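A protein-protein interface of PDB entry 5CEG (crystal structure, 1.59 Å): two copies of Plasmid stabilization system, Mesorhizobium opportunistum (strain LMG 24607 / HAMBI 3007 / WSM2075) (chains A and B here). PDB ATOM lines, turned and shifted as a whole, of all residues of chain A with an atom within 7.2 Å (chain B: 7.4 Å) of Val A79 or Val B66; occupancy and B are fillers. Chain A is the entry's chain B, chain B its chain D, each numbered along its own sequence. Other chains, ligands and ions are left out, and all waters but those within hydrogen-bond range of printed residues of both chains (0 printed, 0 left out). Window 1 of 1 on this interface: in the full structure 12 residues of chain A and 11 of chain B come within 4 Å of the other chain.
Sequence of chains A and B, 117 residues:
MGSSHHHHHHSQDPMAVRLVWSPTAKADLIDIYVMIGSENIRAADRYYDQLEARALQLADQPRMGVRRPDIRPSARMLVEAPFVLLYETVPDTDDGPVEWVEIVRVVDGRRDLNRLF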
ATOM      1  N   LEU A  51      24.053 -10.677  22.649  1.00  0.00           N
ATOM      2  CA  LEU A  51      25.254 -10.661  21.819  1.00  0.00           C
ATOM      3  C   LEU A  51      26.498 -10.919  22.670  1.00  0.00           C
ATOM      4  O   LEU A  51      27.401 -11.636  22.246  1.00  0.00           O
ATOM      5  CB  LEU A  51      25.367  -9.336  21.064  1.00  0.00           C
ATOM      6  CG  LEU A  51      24.361  -9.186  19.920  1.00  0.00           C
ATOM      7  CD1 LEU A  51      24.223  -7.727  19.521  1.00  0.00           C
ATOM      8  CD2 LEU A  51      24.791 -10.040  18.708  1.00  0.00           C
ATOM      9  N   ARG A  54      26.599 -14.637  23.413  1.00  0.00           N
ATOM     10  CA  ARG A  54      27.019 -15.445  22.274  1.00  0.00           C
ATOM     11  C   ARG A  54      28.533 -15.315  22.068  1.00  0.00           C
ATOM     12  O   ARG A  54      29.204 -16.293  21.735  1.00  0.00           O
ATOM     13  CB  ARG A  54      26.262 -15.032  20.999  1.00  0.00           C
ATOM     14  CG  ARG A  54      26.301 -16.063  19.854  1.00  0.00           C
ATOM     15  CD  ARG A  54      25.572 -17.365  20.218  1.00  0.00           C
ATOM     16  NE  ARG A  54      25.055 -18.069  19.039  1.00  0.00           N
ATOM     17  CZ  ARG A  54      24.884 -19.391  18.961  1.00  0.00           C
ATOM     18  NH1 ARG A  54      25.192 -20.163  19.997  1.00  0.00           N
ATOM     19  NH2 ARG A  54      24.388 -19.935  17.848  1.00  0.00           N
ATOM     20  N   GLN A  57      30.375 -17.450  24.625  1.00  0.00           N
ATOM     21  CA  GLN A  57      30.370 -18.839  24.173  1.00  0.00           C
ATOM     22  C   GLN A  57      31.464 -19.087  23.151  1.00  0.00           C
ATOM     23  O   GLN A  57      32.149 -20.111  23.167  1.00  0.00           O
ATOM     24  CB  GLN A  57      29.029 -19.215  23.533  1.00  0.00           C
ATOM     25  CG  GLN A  57      27.879 -19.436  24.470  1.00  0.00           C
ATOM     26  CD  GLN A  57      26.675 -19.963  23.716  1.00  0.00           C
ATOM     27  OE1 GLN A  57      26.373 -19.498  22.618  1.00  0.00           O
ATOM     28  NE2 GLN A  57      25.999 -20.950  24.287  1.00  0.00           N
ATOM     29  N   GLY A  65      31.046 -21.570  14.992  1.00  0.00           N
ATOM     30  CA  GLY A  65      30.446 -21.000  13.799  1.00  0.00           C
ATOM     31  C   GLY A  65      30.679 -21.854  12.556  1.00  0.00           C
ATOM     32  O   GLY A  65      31.739 -22.456  12.388  1.00  0.00           O
ATOM     33  N   VAL A  66      29.680 -21.913  11.685  1.00  0.00           N
ATOM     34  CA  VAL A  66      29.788 -22.677  10.447  1.00  0.00           C
ATOM     35  C   VAL A  66      30.688 -21.966   9.444  1.00  0.00           C
ATOM     36  O   VAL A  66      30.569 -20.755   9.251  1.00  0.00           O
ATOM     37  CB  VAL A  66      28.394 -22.906   9.825  1.00  0.00           C
ATOM     38  CG1 VAL A  66      28.513 -23.429   8.408  1.00  0.00           C
ATOM     39  CG2 VAL A  66      27.576 -23.857  10.704  1.00  0.00           C
ATOM     40  N   MET A  77      30.242 -18.111  10.309  1.00  0.00           N
ATOM     41  CA  MET A  77      29.021 -17.392  10.646  1.00  0.00           C
ATOM     42  C   MET A  77      28.395 -18.006  11.884  1.00  0.00           C
ATOM     43  O   MET A  77      28.255 -19.230  11.970  1.00  0.00           O
ATOM     44  CB  MET A  77      28.055 -17.435   9.456  1.00  0.00           C
ATOM     45  CG  MET A  77      26.676 -16.968   9.759  1.00  0.00           C
ATOM     46  SD  MET A  77      25.630 -17.087   8.292  1.00  0.00           S
ATOM     47  CE  MET A  77      26.519 -16.056   7.132  1.00  0.00           C
ATOM     48  N   LEU A  78      28.058 -17.166  12.858  1.00  0.00           N
ATOM     49  CA  LEU A  78      27.350 -17.616  14.046  1.00  0.00           C
ATOM     50  C   LEU A  78      26.098 -16.762  14.175  1.00  0.00           C
ATOM     51  O   LEU A  78      26.176 -15.539  14.165  1.00  0.00           O
ATOM     52  CB  LEU A  78      28.257 -17.511  15.285  1.00  0.00           C
ATOM     53  CG  LEU A  78      27.794 -18.155  16.591  1.00  0.00           C
ATOM     54  CD1 LEU A  78      27.539 -19.651  16.431  1.00  0.00           C
ATOM     55  CD2 LEU A  78      28.819 -17.891  17.684  1.00  0.00           C
ATOM     56  N   VAL A  79      24.933 -17.401  14.259  1.00  0.00           N
ATOM     57  CA  VAL A  79      23.678 -16.660  14.289  1.00  0.00           C
ATOM     58  C   VAL A  79      23.244 -16.347  15.724  1.00  0.00           C
ATOM     59  O   VAL A  79      23.347 -17.187  16.622  1.00  0.00           O
ATOM     60  CB  VAL A  79      22.552 -17.441  13.545  1.00  0.00           C
ATOM     61  CG1 VAL A  79      21.203 -16.725  13.664  1.00  0.00           C
ATOM     62  CG2 VAL A  79      22.912 -17.619  12.085  1.00  0.00           C
ATOM     63  N   GLU A  80      22.804 -15.107  15.927  1.00  0.00           N
ATOM     64  CA  GLU A  80      22.143 -14.668  17.149  1.00  0.00           C
ATOM     65  C   GLU A  80      20.982 -13.797  16.700  1.00  0.00           C
ATOM     66  O   GLU A  80      21.111 -12.575  16.586  1.00  0.00           O
ATOM     67  CB  GLU A  80      23.109 -13.906  18.068  1.00  0.00           C
ATOM     68  CG  GLU A  80      22.475 -13.381  19.357  1.00  0.00           C
ATOM     69  CD  GLU A  80      21.859 -14.482  20.188  1.00  0.00           C
ATOM     70  OE1 GLU A  80      22.510 -15.541  20.349  1.00  0.00           O
ATOM     71  OE2 GLU A  80      20.726 -14.292  20.673  1.00  0.00           O
ATOM     72  N   ALA A  81      19.852 -14.439  16.407  1.00  0.00           N
ATOM     73  CA  ALA A  81      18.755 -13.786  15.701  1.00  0.00           C
ATOM     74  C   ALA A  81      18.345 -12.462  16.338  1.00  0.00           C
ATOM     75  O   ALA A  81      18.214 -12.379  17.567  1.00  0.00           O
ATOM     76  CB  ALA A  81      17.554 -14.724  15.631  1.00  0.00           C
ATOM     77  N   PRO A  82      18.135 -11.426  15.517  1.00  0.00           N
ATOM     78  CA  PRO A  82      18.163 -11.349  14.045  1.00  0.00           C
ATOM     79  C   PRO A  82      19.536 -11.039  13.434  1.00  0.00           C
ATOM     80  O   PRO A  82      19.620 -10.644  12.258  1.00  0.00           O
ATOM     81  CB  PRO A  82      17.198 -10.195  13.760  1.00  0.00           C
ATOM     82  CG  PRO A  82      17.440  -9.272  14.926  1.00  0.00           C
ATOM     83  CD  PRO A  82      17.640 -10.170  16.113  1.00  0.00           C
ATOM     84  N   PHE A  83      20.593 -11.202  14.225  1.00  0.00           N
ATOM     85  CA  PHE A  83      21.941 -10.843  13.796  1.00  0.00           C
ATOM     86  C   PHE A  83      22.744 -12.047  13.343  1.00  0.00           C
ATOM     87  O   PHE A  83      22.509 -13.182  13.760  1.00  0.00           O
ATOM     88  CB  PHE A  83      22.695 -10.123  14.927  1.00  0.00           C
ATOM     89  CG  PHE A  83      21.908  -9.018  15.549  1.00  0.00           C
ATOM     90  CD1 PHE A  83      21.714  -7.828  14.868  1.00  0.00           C
ATOM     91  CD2 PHE A  83      21.330  -9.186  16.797  1.00  0.00           C
ATOM     92  CE1 PHE A  83      20.970  -6.812  15.432  1.00  0.00           C
ATOM     93  CE2 PHE A  83      20.586  -8.178  17.367  1.00  0.00           C
ATOM     94  CZ  PHE A  83      20.393  -6.997  16.688  1.00  0.00           C
ATOM     95  N   VAL A  84      23.707 -11.776  12.474  1.00  0.00           N
ATOM     96  CA  VAL A  84      24.666 -12.765  12.040  1.00  0.00           C
ATOM     97  C   VAL A  84      26.045 -12.254  12.437  1.00  0.00           C
ATOM     98  O   VAL A  84      26.427 -11.146  12.050  1.00  0.00           O
ATOM     99  CB  VAL A  84      24.572 -12.969  10.515  1.00  0.00           C
ATOM    100  CG1 VAL A  84      25.712 -13.788  10.017  1.00  0.00           C
ATOM    101  CG2 VAL A  84      23.213 -13.596  10.137  1.00  0.00           C
ATOM    102  N   LEU A  85      26.769 -13.027  13.240  1.00  0.00           N
ATOM    103  CA  LEU A  85      28.141 -12.663  13.570  1.00  0.00           C
ATOM    104  C   LEU A  85      29.057 -13.266  12.521  1.00  0.00           C
ATOM    105  O   LEU A  85      29.036 -14.472  12.312  1.00  0.00           O
ATOM    106  CB  LEU A  85      28.543 -13.171  14.958  1.00  0.00           C
ATOM    107  CG  LEU A  85      27.836 -12.688  16.228  1.00  0.00           C
ATOM    108  CD1 LEU A  85      28.408 -13.418  17.433  1.00  0.00           C
ATOM    109  CD2 LEU A  85      27.985 -11.202  16.426  1.00  0.00           C
ATOM    110  N   LEU A 116      17.522 -14.157   4.273  1.00  0.00           N
ATOM    111  CA  LEU A 116      17.408 -14.447   5.701  1.00  0.00           C
ATOM    112  C   LEU A 116      16.751 -13.286   6.433  1.00  0.00           C
ATOM    113  O   LEU A 116      16.954 -12.121   6.063  1.00  0.00           O
ATOM    114  CB  LEU A 116      18.784 -14.714   6.335  1.00  0.00           C
ATOM    115  CG  LEU A 116      19.581 -15.972   5.997  1.00  0.00           C
ATOM    116  CD1 LEU A 116      20.794 -16.037   6.908  1.00  0.00           C
ATOM    117  CD2 LEU A 116      18.743 -17.229   6.144  1.00  0.00           C
ATOM    118  N   PHE A 117      15.961 -13.603   7.460  1.00  0.00           N
ATOM    119  CA  PHE A 117      15.254 -12.602   8.269  1.00  0.00           C
ATOM    120  C   PHE A 117      14.491 -11.572   7.411  1.00  0.00           C
ATOM    121  O   PHE A 117      14.665 -10.361   7.549  1.00  0.00           O
ATOM    122  CB  PHE A 117      16.244 -11.911   9.214  1.00  0.00           C
ATOM    123  CG  PHE A 117      16.922 -12.865  10.167  1.00  0.00           C
ATOM    124  CD1 PHE A 117      16.215 -13.438  11.214  1.00  0.00           C
ATOM    125  CD2 PHE A 117      18.252 -13.210   9.998  1.00  0.00           C
ATOM    126  CE1 PHE A 117      16.823 -14.331  12.081  1.00  0.00           C
ATOM    127  CE2 PHE A 117      18.872 -14.098  10.867  1.00  0.00           C
ATOM    128  CZ  PHE A 117      18.154 -14.660  11.909  1.00  0.00           C
ATOM    129  N   ARG B  63      26.034 -26.633  21.481  1.00  0.00           N
ATOM    130  CA  ARG B  63      25.164 -25.469  21.476  1.00  0.00           C
ATOM    131  C   ARG B  63      25.467 -24.553  20.286  1.00  0.00           C
ATOM    132  O   ARG B  63      25.139 -23.367  20.300  1.00  0.00           O
ATOM    133  CB  ARG B  63      25.284 -24.715  22.822  1.00  0.00           C
ATOM    134  CG  ARG B  63      24.800 -25.546  24.023  1.00  0.00           C
ATOM    135  CD  ARG B  63      24.860 -24.779  25.346  1.00  0.00           C
ATOM    136  NE  ARG B  63      24.342 -25.571  26.466  1.00  0.00           N
ATOM    137  CZ  ARG B  63      25.096 -26.297  27.289  1.00  0.00           C
ATOM    138  NH1 ARG B  63      24.541 -26.981  28.284  1.00  0.00           N
ATOM    139  NH2 ARG B  63      26.410 -26.344  27.121  1.00  0.00           N
ATOM    140  N   MET B  64      26.054 -25.116  19.222  1.00  0.00           N
ATOM    141  CA  MET B  64      26.453 -24.307  18.073  1.00  0.00           C
ATOM    142  C   MET B  64      25.256 -23.918  17.215  1.00  0.00           C
ATOM    143  O   MET B  64      25.321 -22.963  16.456  1.00  0.00           O
ATOM    144  CB  MET B  64      27.494 -25.036  17.205  1.00  0.00           C
ATOM    145  CG  MET B  64      26.979 -26.277  16.493  1.00  0.00           C
ATOM    146  SD  MET B  64      28.313 -27.123  15.589  1.00  0.00           S
ATOM    147  CE  MET B  64      28.558 -25.990  14.227  1.00  0.00           C
ATOM    148  N   GLY B  65      24.165 -24.653  17.350  1.00  0.00           N
ATOM    149  CA  GLY B  65      22.966 -24.313  16.615  1.00  0.00           C
ATOM    150  C   GLY B  65      22.292 -23.094  17.214  1.00  0.00           C
ATOM    151  O   GLY B  65      22.783 -22.470  18.163  1.00  0.00           O
ATOM    152  N   VAL B  66      21.168 -22.734  16.627  1.00  0.00           N
ATOM    153  CA  VAL B  66      20.329 -21.642  17.101  1.00  0.00           C
ATOM    154  C   VAL B  66      19.140 -22.191  17.879  1.00  0.00           C
ATOM    155  O   VAL B  66      18.467 -23.087  17.390  1.00  0.00           O
ATOM    156  CB  VAL B  66      19.818 -20.807  15.906  1.00  0.00           C
ATOM    157  CG1 VAL B  66      18.738 -19.837  16.332  1.00  0.00           C
ATOM    158  CG2 VAL B  66      20.970 -20.072  15.264  1.00  0.00           C
ATOM    159  N   ARG B  67      18.857 -21.660  19.069  1.00  0.00           N
ATOM    160  CA  ARG B  67      17.645 -22.061  19.780  1.00  0.00           C
ATOM    161  C   ARG B  67      16.403 -21.626  19.004  1.00  0.00           C
ATOM    162  O   ARG B  67      16.335 -20.501  18.502  1.00  0.00           O
ATOM    163  CB  ARG B  67      17.606 -21.460  21.189  1.00  0.00           C
ATOM    164  CG  ARG B  67      18.319 -22.267  22.275  1.00  0.00           C
ATOM    165  CD  ARG B  67      17.750 -21.877  23.628  1.00  0.00           C
ATOM    166  NE  ARG B  67      18.363 -22.559  24.762  1.00  0.00           N
ATOM    167  CZ  ARG B  67      18.085 -23.803  25.139  1.00  0.00           C
ATOM    168  NH1 ARG B  67      17.225 -24.541  24.447  1.00  0.00           N
ATOM    169  NH2 ARG B  67      18.684 -24.313  26.210  1.00  0.00           N
ATOM    170  N   ARG B  68      15.418 -22.521  18.922  1.00  0.00           N
ATOM    171  CA  ARG B  68      14.128 -22.211  18.304  1.00  0.00           C
ATOM    172  C   ARG B  68      12.963 -22.650  19.191  1.00  0.00           C
ATOM    173  O   ARG B  68      12.193 -23.556  18.831  1.00  0.00           O
ATOM    174  CB  ARG B  68      14.008 -22.883  16.929  1.00  0.00           C
ATOM    175  CG  ARG B  68      14.951 -22.358  15.861  1.00  0.00           C
ATOM    176  CD  ARG B  68      14.739 -20.874  15.580  1.00  0.00           C
ATOM    177  NE  ARG B  68      13.357 -20.541  15.220  1.00  0.00           N
ATOM    178  CZ  ARG B  68      12.914 -20.413  13.973  1.00  0.00           C
ATOM    179  NH1 ARG B  68      13.737 -20.599  12.948  1.00  0.00           N
ATOM    180  NH2 ARG B  68      11.646 -20.098  13.750  1.00  0.00           N
ATOM    181  N   PRO B  69      12.805 -22.009  20.357  1.00  0.00           N
ATOM    182  CA  PRO B  69      11.730 -22.400  21.263  1.00  0.00           C
ATOM    183  C   PRO B  69      10.364 -22.086  20.670  1.00  0.00           C
ATOM    184  O   PRO B  69       9.366 -22.569  21.205  1.00  0.00           O
ATOM    185  CB  PRO B  69      12.001 -21.551  22.523  1.00  0.00           C
ATOM    186  CG  PRO B  69      12.759 -20.375  22.015  1.00  0.00           C
ATOM    187  CD  PRO B  69      13.633 -20.927  20.924  1.00  0.00           C
ATOM    188  N   ILE B  71       9.503 -23.212  17.896  1.00  0.00           N
ATOM    189  CA  ILE B  71       9.124 -24.498  17.299  1.00  0.00           C
ATOM    190  C   ILE B  71       8.655 -25.441  18.414  1.00  0.00           C
ATOM    191  O   ILE B  71       7.472 -25.751  18.512  1.00  0.00           O
ATOM    192  CB  ILE B  71      10.292 -25.127  16.502  1.00  0.00           C
ATOM    193  CG1 ILE B  71      10.716 -24.202  15.357  1.00  0.00           C
ATOM    194  CG2 ILE B  71       9.903 -26.510  15.958  1.00  0.00           C
ATOM    195  CD1 ILE B  71      11.925 -24.706  14.569  1.00  0.00           C
ATOM    196  N   SER B  74      12.734 -27.152  23.473  1.00  0.00           N
ATOM    197  CA  SER B  74      14.125 -27.606  23.441  1.00  0.00           C
ATOM    198  C   SER B  74      14.749 -27.594  22.039  1.00  0.00           C
ATOM    199  O   SER B  74      15.914 -27.955  21.869  1.00  0.00           O
ATOM    200  CB  SER B  74      14.225 -29.020  24.017  1.00  0.00           C
ATOM    201  OG  SER B  74      13.633 -29.960  23.132  1.00  0.00           O
ATOM    202  N   ALA B  75      13.981 -27.182  21.036  1.00  0.00           N
ATOM    203  CA  ALA B  75      14.440 -27.298  19.658  1.00  0.00           C
ATOM    204  C   ALA B  75      15.573 -26.338  19.324  1.00  0.00           C
ATOM    205  O   ALA B  75      15.581 -25.171  19.752  1.00  0.00           O
ATOM    206  CB  ALA B  75      13.266 -27.087  18.690  1.00  0.00           C
ATOM    207  N   ARG B  76      16.531 -26.851  18.557  1.00  0.00           N
ATOM    208  CA  ARG B  76      17.627 -26.061  18.004  1.00  0.00           C
ATOM    209  C   ARG B  76      17.761 -26.391  16.522  1.00  0.00           C
ATOM    210  O   ARG B  76      17.405 -27.491  16.100  1.00  0.00           O
ATOM    211  CB  ARG B  76      18.946 -26.351  18.731  1.00  0.00           C
ATOM    212  CG  ARG B  76      18.905 -26.077  20.251  1.00  0.00           C
ATOM    213  CD  ARG B  76      20.303 -26.229  20.869  1.00  0.00           C
ATOM    214  NE  ARG B  76      20.272 -26.547  22.302  1.00  0.00           N
ATOM    215  CZ  ARG B  76      20.744 -25.758  23.267  1.00  0.00           C
ATOM    216  NH1 ARG B  76      21.268 -24.582  22.957  1.00  0.00           N
ATOM    217  NH2 ARG B  76      20.686 -26.148  24.548  1.00  0.00           N
ATOM    218  N   MET B  77      18.269 -25.437  15.742  1.00  0.00           N
ATOM    219  CA  MET B  77      18.481 -25.610  14.304  1.00  0.00           C
ATOM    220  C   MET B  77      19.948 -25.425  13.969  1.00  0.00           C
ATOM    221  O   MET B  77      20.571 -24.455  14.406  1.00  0.00           O
ATOM    222  CB  MET B  77      17.666 -24.584  13.496  1.00  0.00           C
ATOM    223  CG  MET B  77      16.204 -24.912  13.321  1.00  0.00           C
ATOM    224  SD  MET B  77      15.348 -23.591  12.421  1.00  0.00           S
ATOM    225  CE  MET B  77      16.468 -23.396  11.039  1.00  0.00           C
ATOM    226  N   LEU B  78      20.501 -26.340  13.181  1.00  0.00           N
ATOM    227  CA  LEU B  78      21.858 -26.188  12.672  1.00  0.00           C
ATOM    228  C   LEU B  78      21.834 -26.406  11.170  1.00  0.00           C
ATOM    229  O   LEU B  78      21.472 -27.482  10.712  1.00  0.00           O
ATOM    230  CB  LEU B  78      22.803 -27.187  13.338  1.00  0.00           C
ATOM    231  CG  LEU B  78      24.244 -27.182  12.826  1.00  0.00           C
ATOM    232  CD1 LEU B  78      24.878 -25.798  12.975  1.00  0.00           C
ATOM    233  CD2 LEU B  78      25.047 -28.232  13.578  1.00  0.00           C
ATOM    234  N   VAL B  79      22.231 -25.399  10.406  1.00  0.00           N
ATOM    235  CA  VAL B  79      22.209 -25.509   8.950  1.00  0.00           C
ATOM    236  C   VAL B  79      23.397 -26.333   8.427  1.00  0.00           C
ATOM    237  O   VAL B  79      24.511 -26.255   8.949  1.00  0.00           O
ATOM    238  CB  VAL B  79      22.196 -24.105   8.310  1.00  0.00           C
ATOM    239  CG1 VAL B  79      22.315 -24.180   6.793  1.00  0.00           C
ATOM    240  CG2 VAL B  79      20.930 -23.366   8.712  1.00  0.00           C
ATOM    241  N   LEU B  85      19.493 -29.432  10.328  1.00  0.00           N
ATOM    242  CA  LEU B  85      19.399 -30.428  11.386  1.00  0.00           C
ATOM    243  C   LEU B  85      18.559 -29.842  12.501  1.00  0.00           C
ATOM    244  O   LEU B  85      18.893 -28.779  13.023  1.00  0.00           O
ATOM    245  CB  LEU B  85      20.779 -30.799  11.923  1.00  0.00           C
ATOM    246  CG  LEU B  85      21.830 -31.272  10.920  1.00  0.00           C
ATOM    247  CD1 LEU B  85      23.176 -31.447  11.618  1.00  0.00           C
ATOM    248  CD2 LEU B  85      21.389 -32.567  10.301  1.00  0.00           C
ATOM    249  N   TYR B  87      17.579 -30.412  16.282  1.00  0.00           N
ATOM    250  CA  TYR B  87      18.137 -31.231  17.352  1.00  0.00           C
ATOM    251  C   TYR B  87      17.869 -30.642  18.719  1.00  0.00           C
ATOM    252  O   TYR B  87      17.429 -29.495  18.842  1.00  0.00           O
ATOM    253  CB  TYR B  87      19.652 -31.414  17.153  1.00  0.00           C
ATOM    254  CG  TYR B  87      20.528 -30.239  17.568  1.00  0.00           C
ATOM    255  CD1 TYR B  87      20.772 -29.173  16.701  1.00  0.00           C
ATOM    256  CD2 TYR B  87      21.129 -30.209  18.818  1.00  0.00           C
ATOM    257  CE1 TYR B  87      21.580 -28.104  17.085  1.00  0.00           C
ATOM    258  CE2 TYR B  87      21.944 -29.148  19.205  1.00  0.00           C
ATOM    259  CZ  TYR B  87      22.164 -28.102  18.340  1.00  0.00           C
ATOM    260  OH  TYR B  87      22.984 -27.049  18.726  1.00  0.00           O
ATOM    261  N   PHE B 117      15.909 -18.837   7.813  1.00  0.00           N
ATOM    262  CA  PHE B 117      15.604 -17.959   8.944  1.00  0.00           C
ATOM    263  C   PHE B 117      14.875 -16.731   8.427  1.00  0.00           C
ATOM    264  O   PHE B 117      15.087 -16.327   7.283  1.00  0.00           O
ATOM    265  CB  PHE B 117      16.870 -17.517   9.688  1.00  0.00           C
ATOM    266  CG  PHE B 117      17.633 -18.636  10.330  1.00  0.00           C
ATOM    267  CD1 PHE B 117      18.931 -18.917   9.939  1.00  0.00           C
ATOM    268  CD2 PHE B 117      17.062 -19.394  11.334  1.00  0.00           C
ATOM    269  CE1 PHE B 117      19.647 -19.944  10.536  1.00  0.00           C
ATOM    270  CE2 PHE B 117      17.771 -20.418  11.937  1.00  0.00           C
ATOM    271  CZ  PHE B 117      19.064 -20.698  11.534  1.00  0.00           C
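NH1 of Arg A54 sits at hydrogen-bond distance from O of Arg B63, 3.2 Å away. The backbone carbonyl oxygen (O) of Met B64 sits at hydrogen-bond distance from the guanidinium group (NH2) of Arg A54, 3.5 Å away. NH2 of Arg A54 lies within hydrogen-bond range of O of Gly B65. The backbone NH of Phe A117 sits at hydrogen-bond distance from the backbone carbonyl oxygen of Phe B117 (2.9 Å).
The guanidinium group (NH1) of Arg A54 is in hydrogen-bond range of the side-chain amide oxygen (OE1) of Gln A57, 3.0 Å away. NE of Arg A54 lies within hydrogen-bond range of O of Val A79 (3.1 Å). The side-chain carboxylate of Glu A80 lies within salt-bridge range of the guanidinium group of Arg A54 (3.8 Å). The backbone NH of Leu A85 sits at hydrogen-bond distance from the backbone carbonyl oxygen of Leu A78. N of Gly B65 sits at hydrogen-bond distance from OH of Tyr B87 (3.0 Å). The backbone NH of Val B66 lies within hydrogen-bond range of the backbone carbonyl oxygen of Met B77.
Of the printed residues of chain B, Arg A54 touches Arg B63 (3.2 Å), Met B64 (3.5 Å) and Gly B65 (3.0 Å). Printed residues of chain B within 4 Å of Val A79: Val B66. Pro A82 touches none of the printed residues of chain B. Printed residues of chain A within 4 Å of Arg B63: Arg A54 (3.2 Å). Of the printed residues of chain A, Gly B65 touches Arg A54 (3.0 Å). Of the printed residues of chain A, Val B66 touches Val A79 (3.5 Å). The nearest printed residue of chain B that does not touch Val A79 is Phe B117 (4.3 Å). The nearest printed residue of chain A that does not touch Val B66 is Arg A54 (4.3 Å). The nearest printed residue of chain B that does not touch Leu A78 is Gly B65 (5.8 Å).
Hydrophobic or aromatic side chains of chain A that line the printed part of chain B: Leu A78, Val A79, Leu A116 and Phe A117. Among the printed residues, 7 pairs touch across the chains.
Val A79 touches Val B66, but with the chains exchanged Val A66 does not touch Val B79 (4.3 Å). Phe B117 touches its own counterpart, Phe A117. 7 positions are printed for both chains. Of the 7 pairs that touch across the chains among the printed residues, 1 has its exchanged pair printed and touching as well.
Among the printed residues, merely in contact across the chains: Leu A78 with Met B64, Val A79 with Val B66 and Leu A116 with Phe B117.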
